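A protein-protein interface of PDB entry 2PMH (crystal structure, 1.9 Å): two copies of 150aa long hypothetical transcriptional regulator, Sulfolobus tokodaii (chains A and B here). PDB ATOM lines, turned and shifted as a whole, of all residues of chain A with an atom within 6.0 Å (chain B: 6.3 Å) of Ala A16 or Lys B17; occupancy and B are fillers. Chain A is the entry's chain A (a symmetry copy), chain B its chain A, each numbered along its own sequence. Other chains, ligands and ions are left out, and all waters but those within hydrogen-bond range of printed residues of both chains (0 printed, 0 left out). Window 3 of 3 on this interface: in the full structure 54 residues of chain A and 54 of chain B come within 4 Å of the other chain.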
ATOM      1  N   ILE A  11      10.348  -6.271 -12.916  1.00  0.00           N
ATOM      2  CA  ILE A  11       9.985  -5.327 -11.866  1.00  0.00           C
ATOM      3  C   ILE A  11       9.949  -6.028 -10.509  1.00  0.00           C
ATOM      4  O   ILE A  11      10.521  -5.550  -9.529  1.00  0.00           O
ATOM      5  CB  ILE A  11       8.582  -4.712 -12.117  1.00  0.00           C
ATOM      6  CG1 ILE A  11       8.615  -3.825 -13.362  1.00  0.00           C
ATOM      7  CG2 ILE A  11       8.135  -3.918 -10.900  1.00  0.00           C
ATOM      8  CD1 ILE A  11       7.275  -3.198 -13.707  1.00  0.00           C
ATOM      9  N   LEU A  12       9.268  -7.167 -10.463  1.00  0.00           N
ATOM     10  CA  LEU A  12       9.121  -7.914  -9.225  1.00  0.00           C
ATOM     11  C   LEU A  12      10.428  -8.460  -8.666  1.00  0.00           C
ATOM     12  O   LEU A  12      10.532  -8.713  -7.471  1.00  0.00           O
ATOM     13  CB  LEU A  12       8.110  -9.041  -9.415  1.00  0.00           C
ATOM     14  CG  LEU A  12       6.715  -8.566  -9.847  1.00  0.00           C
ATOM     15  CD1 LEU A  12       5.750  -9.743  -9.850  1.00  0.00           C
ATOM     16  CD2 LEU A  12       6.214  -7.486  -8.900  1.00  0.00           C
ATOM     17  N   GLN A  13      11.425  -8.630  -9.529  1.00  0.00           N
ATOM     18  CA  GLN A  13      12.722  -9.142  -9.097  1.00  0.00           C
ATOM     19  C   GLN A  13      13.471  -8.058  -8.312  1.00  0.00           C
ATOM     20  O   GLN A  13      14.351  -8.359  -7.503  1.00  0.00           O
ATOM     21  CB  GLN A  13      13.557  -9.567 -10.312  1.00  0.00           C
ATOM     22  CG  GLN A  13      14.173  -8.408 -11.083  1.00  0.00           C
ATOM     23  CD  GLN A  13      15.013  -8.868 -12.254  1.00  0.00           C
ATOM     24  OE1 GLN A  13      15.405 -10.028 -12.326  1.00  0.00           O
ATOM     25  NE2 GLN A  13      15.303  -7.957 -13.174  1.00  0.00           N
ATOM     26  N   TYR A  14      13.112  -6.804  -8.566  1.00  0.00           N
ATOM     27  CA  TYR A  14      13.734  -5.651  -7.914  1.00  0.00           C
ATOM     28  C   TYR A  14      12.951  -5.175  -6.705  1.00  0.00           C
ATOM     29  O   TYR A  14      13.512  -4.937  -5.633  1.00  0.00           O
ATOM     30  CB  TYR A  14      13.834  -4.482  -8.894  1.00  0.00           C
ATOM     31  CG  TYR A  14      15.120  -4.430  -9.666  1.00  0.00           C
ATOM     32  CD1 TYR A  14      16.319  -4.100  -9.032  1.00  0.00           C
ATOM     33  CD2 TYR A  14      15.150  -4.726 -11.030  1.00  0.00           C
ATOM     34  CE1 TYR A  14      17.525  -4.067  -9.734  1.00  0.00           C
ATOM     35  CE2 TYR A  14      16.352  -4.698 -11.748  1.00  0.00           C
ATOM     36  CZ  TYR A  14      17.536  -4.369 -11.093  1.00  0.00           C
ATOM     37  OH  TYR A  14      18.734  -4.361 -11.779  1.00  0.00           O
ATOM     38  N   ASN A  15      11.648  -5.027  -6.890  1.00  0.00           N
ATOM     39  CA  ASN A  15      10.791  -4.545  -5.825  1.00  0.00           C
ATOM     40  C   ASN A  15       9.440  -5.229  -5.929  1.00  0.00           C
ATOM     41  O   ASN A  15       8.641  -4.900  -6.799  1.00  0.00           O
ATOM     42  CB  ASN A  15      10.610  -3.034  -5.966  1.00  0.00           C
ATOM     43  CG  ASN A  15      10.047  -2.398  -4.713  1.00  0.00           C
ATOM     44  OD1 ASN A  15       9.225  -2.995  -4.012  1.00  0.00           O
ATOM     45  ND2 ASN A  15      10.480  -1.174  -4.426  1.00  0.00           N
ATOM     46  N   ALA A  16       9.191  -6.190  -5.051  1.00  0.00           N
ATOM     47  CA  ALA A  16       7.927  -6.907  -5.074  1.00  0.00           C
ATOM     48  C   ALA A  16       6.889  -6.168  -4.241  1.00  0.00           C
ATOM     49  O   ALA A  16       5.760  -6.631  -4.099  1.00  0.00           O
ATOM     50  CB  ALA A  16       8.119  -8.313  -4.537  1.00  0.00           C
ATOM     51  N   LYS A  17       7.274  -5.016  -3.697  1.00  0.00           N
ATOM     52  CA  LYS A  17       6.372  -4.221  -2.867  1.00  0.00           C
ATOM     53  C   LYS A  17       5.736  -3.060  -3.631  1.00  0.00           C
ATOM     54  O   LYS A  17       5.250  -2.108  -3.024  1.00  0.00           O
ATOM     55  CB  LYS A  17       7.120  -3.682  -1.642  1.00  0.00           C
ATOM     56  CG  LYS A  17       6.337  -3.797  -0.339  1.00  0.00           C
ATOM     57  CD  LYS A  17       6.037  -5.260   0.003  1.00  0.00           C
ATOM     58  CE  LYS A  17       5.289  -5.388   1.327  1.00  0.00           C
ATOM     59  NZ  LYS A  17       4.998  -6.810   1.659  1.00  0.00           N
ATOM     60  N   TYR A  18       5.754  -3.133  -4.959  1.00  0.00           N
ATOM     61  CA  TYR A  18       5.151  -2.096  -5.788  1.00  0.00           C
ATOM     62  C   TYR A  18       3.643  -2.271  -5.771  1.00  0.00           C
ATOM     63  O   TYR A  18       3.141  -3.352  -5.461  1.00  0.00           O
ATOM     64  CB  TYR A  18       5.632  -2.208  -7.232  1.00  0.00           C
ATOM     65  CG  TYR A  18       6.812  -1.341  -7.581  1.00  0.00           C
ATOM     66  CD1 TYR A  18       6.727   0.050  -7.512  1.00  0.00           C
ATOM     67  CD2 TYR A  18       8.006  -1.908  -8.016  1.00  0.00           C
ATOM     68  CE1 TYR A  18       7.807   0.855  -7.877  1.00  0.00           C
ATOM     69  CE2 TYR A  18       9.091  -1.118  -8.382  1.00  0.00           C
ATOM     70  CZ  TYR A  18       8.986   0.261  -8.310  1.00  0.00           C
ATOM     71  OH  TYR A  18      10.064   1.034  -8.677  1.00  0.00           O
ATOM     72  N   GLU A  42       2.884 -17.613 -10.591  1.00  0.00           N
ATOM     73  CA  GLU A  42       3.115 -18.261  -9.308  1.00  0.00           C
ATOM     74  C   GLU A  42       2.763 -19.743  -9.369  1.00  0.00           C
ATOM     75  O   GLU A  42       3.521 -20.591  -8.894  1.00  0.00           O
ATOM     76  CB  GLU A  42       2.297 -17.571  -8.216  1.00  0.00           C
ATOM     77  CG  GLU A  42       2.589 -16.085  -8.082  1.00  0.00           C
ATOM     78  CD  GLU A  42       1.710 -15.410  -7.050  1.00  0.00           C
ATOM     79  OE1 GLU A  42       0.493 -15.692  -7.027  1.00  0.00           O
ATOM     80  OE2 GLU A  42       2.229 -14.589  -6.268  1.00  0.00           O
ATOM     81  N   TYR A  50       8.144 -14.792  -2.459  1.00  0.00           N
ATOM     82  CA  TYR A  50       8.574 -13.423  -2.210  1.00  0.00           C
ATOM     83  C   TYR A  50       9.346 -13.412  -0.901  1.00  0.00           C
ATOM     84  O   TYR A  50       8.896 -13.962   0.106  1.00  0.00           O
ATOM     85  CB  TYR A  50       7.360 -12.498  -2.128  1.00  0.00           C
ATOM     86  CG  TYR A  50       6.519 -12.506  -3.385  1.00  0.00           C
ATOM     87  CD1 TYR A  50       6.835 -11.693  -4.476  1.00  0.00           C
ATOM     88  CD2 TYR A  50       5.411 -13.346  -3.490  1.00  0.00           C
ATOM     89  CE1 TYR A  50       6.062 -11.721  -5.640  1.00  0.00           C
ATOM     90  CE2 TYR A  50       4.636 -13.381  -4.648  1.00  0.00           C
ATOM     91  CZ  TYR A  50       4.966 -12.569  -5.714  1.00  0.00           C
ATOM     92  OH  TYR A  50       4.192 -12.626  -6.848  1.00  0.00           O
ATOM     93  N   LEU B  12       9.965 -13.329   7.450  1.00  0.00           N
ATOM     94  CA  LEU B  12      10.001 -12.539   6.231  1.00  0.00           C
ATOM     95  C   LEU B  12      11.086 -12.957   5.248  1.00  0.00           C
ATOM     96  O   LEU B  12      10.971 -12.699   4.054  1.00  0.00           O
ATOM     97  CB  LEU B  12      10.137 -11.058   6.577  1.00  0.00           C
ATOM     98  CG  LEU B  12       9.003 -10.513   7.458  1.00  0.00           C
ATOM     99  CD1 LEU B  12       9.147  -9.006   7.606  1.00  0.00           C
ATOM    100  CD2 LEU B  12       7.654 -10.848   6.839  1.00  0.00           C
ATOM    101  N   ASN B  15       9.063 -16.066   3.614  1.00  0.00           N
ATOM    102  CA  ASN B  15       7.843 -15.710   2.918  1.00  0.00           C
ATOM    103  C   ASN B  15       7.424 -14.313   3.337  1.00  0.00           C
ATOM    104  O   ASN B  15       6.921 -14.117   4.437  1.00  0.00           O
ATOM    105  CB  ASN B  15       6.742 -16.704   3.286  1.00  0.00           C
ATOM    106  CG  ASN B  15       5.560 -16.637   2.344  1.00  0.00           C
ATOM    107  OD1 ASN B  15       5.200 -15.564   1.853  1.00  0.00           O
ATOM    108  ND2 ASN B  15       4.941 -17.786   2.090  1.00  0.00           N
ATOM    109  N   ALA B  16       7.643 -13.340   2.463  1.00  0.00           N
ATOM    110  CA  ALA B  16       7.281 -11.967   2.775  1.00  0.00           C
ATOM    111  C   ALA B  16       5.833 -11.704   2.383  1.00  0.00           C
ATOM    112  O   ALA B  16       5.342 -10.588   2.529  1.00  0.00           O
ATOM    113  CB  ALA B  16       8.200 -11.009   2.041  1.00  0.00           C
ATOM    114  N   LYS B  17       5.154 -12.737   1.892  1.00  0.00           N
ATOM    115  CA  LYS B  17       3.761 -12.607   1.469  1.00  0.00           C
ATOM    116  C   LYS B  17       2.775 -13.114   2.521  1.00  0.00           C
ATOM    117  O   LYS B  17       1.624 -13.407   2.206  1.00  0.00           O
ATOM    118  CB  LYS B  17       3.538 -13.358   0.152  1.00  0.00           C
ATOM    119  CG  LYS B  17       2.700 -12.589  -0.864  1.00  0.00           C
ATOM    120  CD  LYS B  17       3.383 -11.281  -1.273  1.00  0.00           C
ATOM    121  CE  LYS B  17       2.571 -10.524  -2.320  1.00  0.00           C
ATOM    122  NZ  LYS B  17       3.236  -9.253  -2.719  1.00  0.00           N
ATOM    123  N   TYR B  18       3.231 -13.233   3.765  1.00  0.00           N
ATOM    124  CA  TYR B  18       2.371 -13.680   4.854  1.00  0.00           C
ATOM    125  C   TYR B  18       1.467 -12.532   5.266  1.00  0.00           C
ATOM    126  O   TYR B  18       1.765 -11.369   4.992  1.00  0.00           O
ATOM    127  CB  TYR B  18       3.201 -14.096   6.066  1.00  0.00           C
ATOM    128  CG  TYR B  18       3.515 -15.566   6.149  1.00  0.00           C
ATOM    129  CD1 TYR B  18       2.499 -16.513   6.276  1.00  0.00           C
ATOM    130  CD2 TYR B  18       4.834 -16.011   6.138  1.00  0.00           C
ATOM    131  CE1 TYR B  18       2.792 -17.871   6.397  1.00  0.00           C
ATOM    132  CE2 TYR B  18       5.142 -17.363   6.257  1.00  0.00           C
ATOM    133  CZ  TYR B  18       4.118 -18.287   6.385  1.00  0.00           C
ATOM    134  OH  TYR B  18       4.433 -19.621   6.505  1.00  0.00           O
ATOM    135  N   SER B  19       0.365 -12.860   5.928  1.00  0.00           N
ATOM    136  CA  SER B  19      -0.564 -11.839   6.394  1.00  0.00           C
ATOM    137  C   SER B  19      -0.129 -11.393   7.787  1.00  0.00           C
ATOM    138  O   SER B  19       0.350 -12.202   8.583  1.00  0.00           O
ATOM    139  CB  SER B  19      -1.989 -12.403   6.446  1.00  0.00           C
ATOM    140  OG  SER B  19      -2.064 -13.524   7.312  1.00  0.00           O
ATOM    141  N   GLU B  22      -1.531 -13.567  10.542  1.00  0.00           N
ATOM    142  CA  GLU B  22      -0.896 -14.862  10.721  1.00  0.00           C
ATOM    143  C   GLU B  22       0.455 -14.684  11.411  1.00  0.00           C
ATOM    144  O   GLU B  22       0.829 -15.482  12.273  1.00  0.00           O
ATOM    145  CB  GLU B  22      -0.721 -15.563   9.372  1.00  0.00           C
ATOM    146  CG  GLU B  22      -2.026 -16.065   8.763  1.00  0.00           C
ATOM    147  CD  GLU B  22      -1.817 -16.765   7.430  1.00  0.00           C
ATOM    148  OE1 GLU B  22      -1.345 -16.104   6.477  1.00  0.00           O
ATOM    149  OE2 GLU B  22      -2.124 -17.975   7.336  1.00  0.00           O
ATOM    150  N   TYR B  50      11.974  -6.061  -0.711  1.00  0.00           N
ATOM    151  CA  TYR B  50      11.266  -7.318  -0.911  1.00  0.00           C
ATOM    152  C   TYR B  50      11.390  -7.690  -2.380  1.00  0.00           C
ATOM    153  O   TYR B  50      11.158  -6.866  -3.265  1.00  0.00           O
ATOM    154  CB  TYR B  50       9.798  -7.162  -0.517  1.00  0.00           C
ATOM    155  CG  TYR B  50       9.609  -6.739   0.923  1.00  0.00           C
ATOM    156  CD1 TYR B  50       9.598  -7.675   1.960  1.00  0.00           C
ATOM    157  CD2 TYR B  50       9.459  -5.392   1.252  1.00  0.00           C
ATOM    158  CE1 TYR B  50       9.441  -7.272   3.289  1.00  0.00           C
ATOM    159  CE2 TYR B  50       9.304  -4.982   2.574  1.00  0.00           C
ATOM    160  CZ  TYR B  50       9.296  -5.924   3.584  1.00  0.00           C
ATOM    161  OH  TYR B  50       9.149  -5.496   4.881  1.00  0.00           O
ATOM    162  N   TYR B  51      11.756  -8.941  -2.631  1.00  0.00           N
ATOM    163  CA  TYR B  51      11.965  -9.419  -3.990  1.00  0.00           C
ATOM    164  C   TYR B  51      11.158 -10.659  -4.307  1.00  0.00           C
ATOM    165  O   TYR B  51      10.835 -11.452  -3.426  1.00  0.00           O
ATOM    166  CB  TYR B  51      13.447  -9.774  -4.196  1.00  0.00           C
ATOM    167  CG  TYR B  51      14.437  -8.677  -3.856  1.00  0.00           C
ATOM    168  CD1 TYR B  51      15.760  -8.987  -3.536  1.00  0.00           C
ATOM    169  CD2 TYR B  51      14.068  -7.331  -3.884  1.00  0.00           C
ATOM    170  CE1 TYR B  51      16.692  -7.981  -3.256  1.00  0.00           C
ATOM    171  CE2 TYR B  51      14.991  -6.316  -3.606  1.00  0.00           C
ATOM    172  CZ  TYR B  51      16.300  -6.649  -3.296  1.00  0.00           C
ATOM    173  OH  TYR B  51      17.212  -5.648  -3.048  1.00  0.00           O
ATOM    174  N   ALA B  52      10.853 -10.831  -5.585  1.00  0.00           N
ATOM    175  CA  ALA B  52      10.147 -12.018  -6.035  1.00  0.00           C
ATOM    176  C   ALA B  52      11.245 -13.022  -6.382  1.00  0.00           C
ATOM    177  O   ALA B  52      12.199 -12.682  -7.080  1.00  0.00           O
ATOM    178  CB  ALA B  52       9.320 -11.706  -7.270  1.00  0.00           C
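The side-chain amide oxygen (OD1) of Asn B15 sits at hydrogen-bond distance from the backbone NH (N) of Lys B17, 2.8 Å away. The side-chain amide oxygen of Asn A15 lies within hydrogen-bond range of the backbone NH of Lys A17, at 2.8 Å. The side-chain hydroxyl (OH) of Tyr A50 lies within hydrogen-bond range of the side-chain carboxylate (OE2) of Glu A42.
Asn A15 touches Tyr B50, and with the chains exchanged Tyr A50 touches Asn B15. Ala A16 touches Lys B17, and with the chains exchanged Lys A17 touches Ala B16. Ala A16 touches Tyr B50, and with the chains exchanged Tyr A50 touches Ala B16. Lys A17 touches Tyr B50, and with the chains exchanged Tyr A50 touches Lys B17. Of the 17 pairs that touch across the chains among the printed residues, 8 have their exchanged pair printed and touching as well.
O of Tyr A50 lies within hydrogen-bond range of N of Ala B16 (2.7 Å). O of Tyr B50 is in hydrogen-bond range of N of Ala A16 (2.7 Å). The backbone NH (N) of Ala B52 is in hydrogen-bond range of the backbone carbonyl oxygen (O) of Leu A12.
Of the 10 printed residues of chain B, 6 touch a printed residue of chain A. Hydrophobic or aromatic side chains of chain B within 4 Å of the printed part of chain A: Ala B16, Tyr B50, Tyr B51 and Ala B52. Along chain B the printed residues that touch a printed residue of chain A span positions 15 to 52. Hydrophobic or aromatic side chains of chain A that line the printed part of chain B: Leu A12, Ala A16 and Tyr A50. Along chain A the printed residues that touch a printed residue of chain B span positions 12 to 50. Among the printed residues, no Asp or Glu carboxylate lies within 4 Å of a Lys or Arg side-chain nitrogen of the other chain.
Gln A13 touches Tyr B51. Tyr A14 touches Tyr B51 (O to CE2, 2.9 Å). Asn A15 touches Tyr B50 (CA to O, 3.5 Å). NZ of Lys B17 touches O of Ala A16, at 3.9 Å. Lys A17 touches Ala B16. Lys A17 touches Tyr B50 (CD to CD2, 3.6 Å). Asn B15 touches Tyr A50 (CA to O, 3.5 Å). CD of Lys B17 touches CD2 of Tyr A50, 3.6 Å away. Tyr B51 touches Tyr A50. Tyr A50 touches Ala B52.
Ile A11 touches none of the printed residues of chain B. Of the printed residues of chain B, Asn A15 touches Tyr B50 (3.5 Å). Ala A16 touches just these residues of chain B: Lys B17, Tyr B50, Tyr B51 and Ala B52. Of the printed residues of chain B, Tyr A50 touches Asn B15, Ala B16, Lys B17, Tyr B51 and Ala B52. Printed residues of chain A within 4 Å of Asn B15: Tyr A50 (3.5 Å). Of the printed residues of chain A, Ala B16 touches Lys A17 (3.9 Å) and Tyr A50 (2.7 Å). Lys B17 touches just these residues of chain A: Ala A16 and Tyr A50. Of the printed residues of chain A, Tyr B50 touches Tyr A14, Asn A15, Ala A16 and Lys A17.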
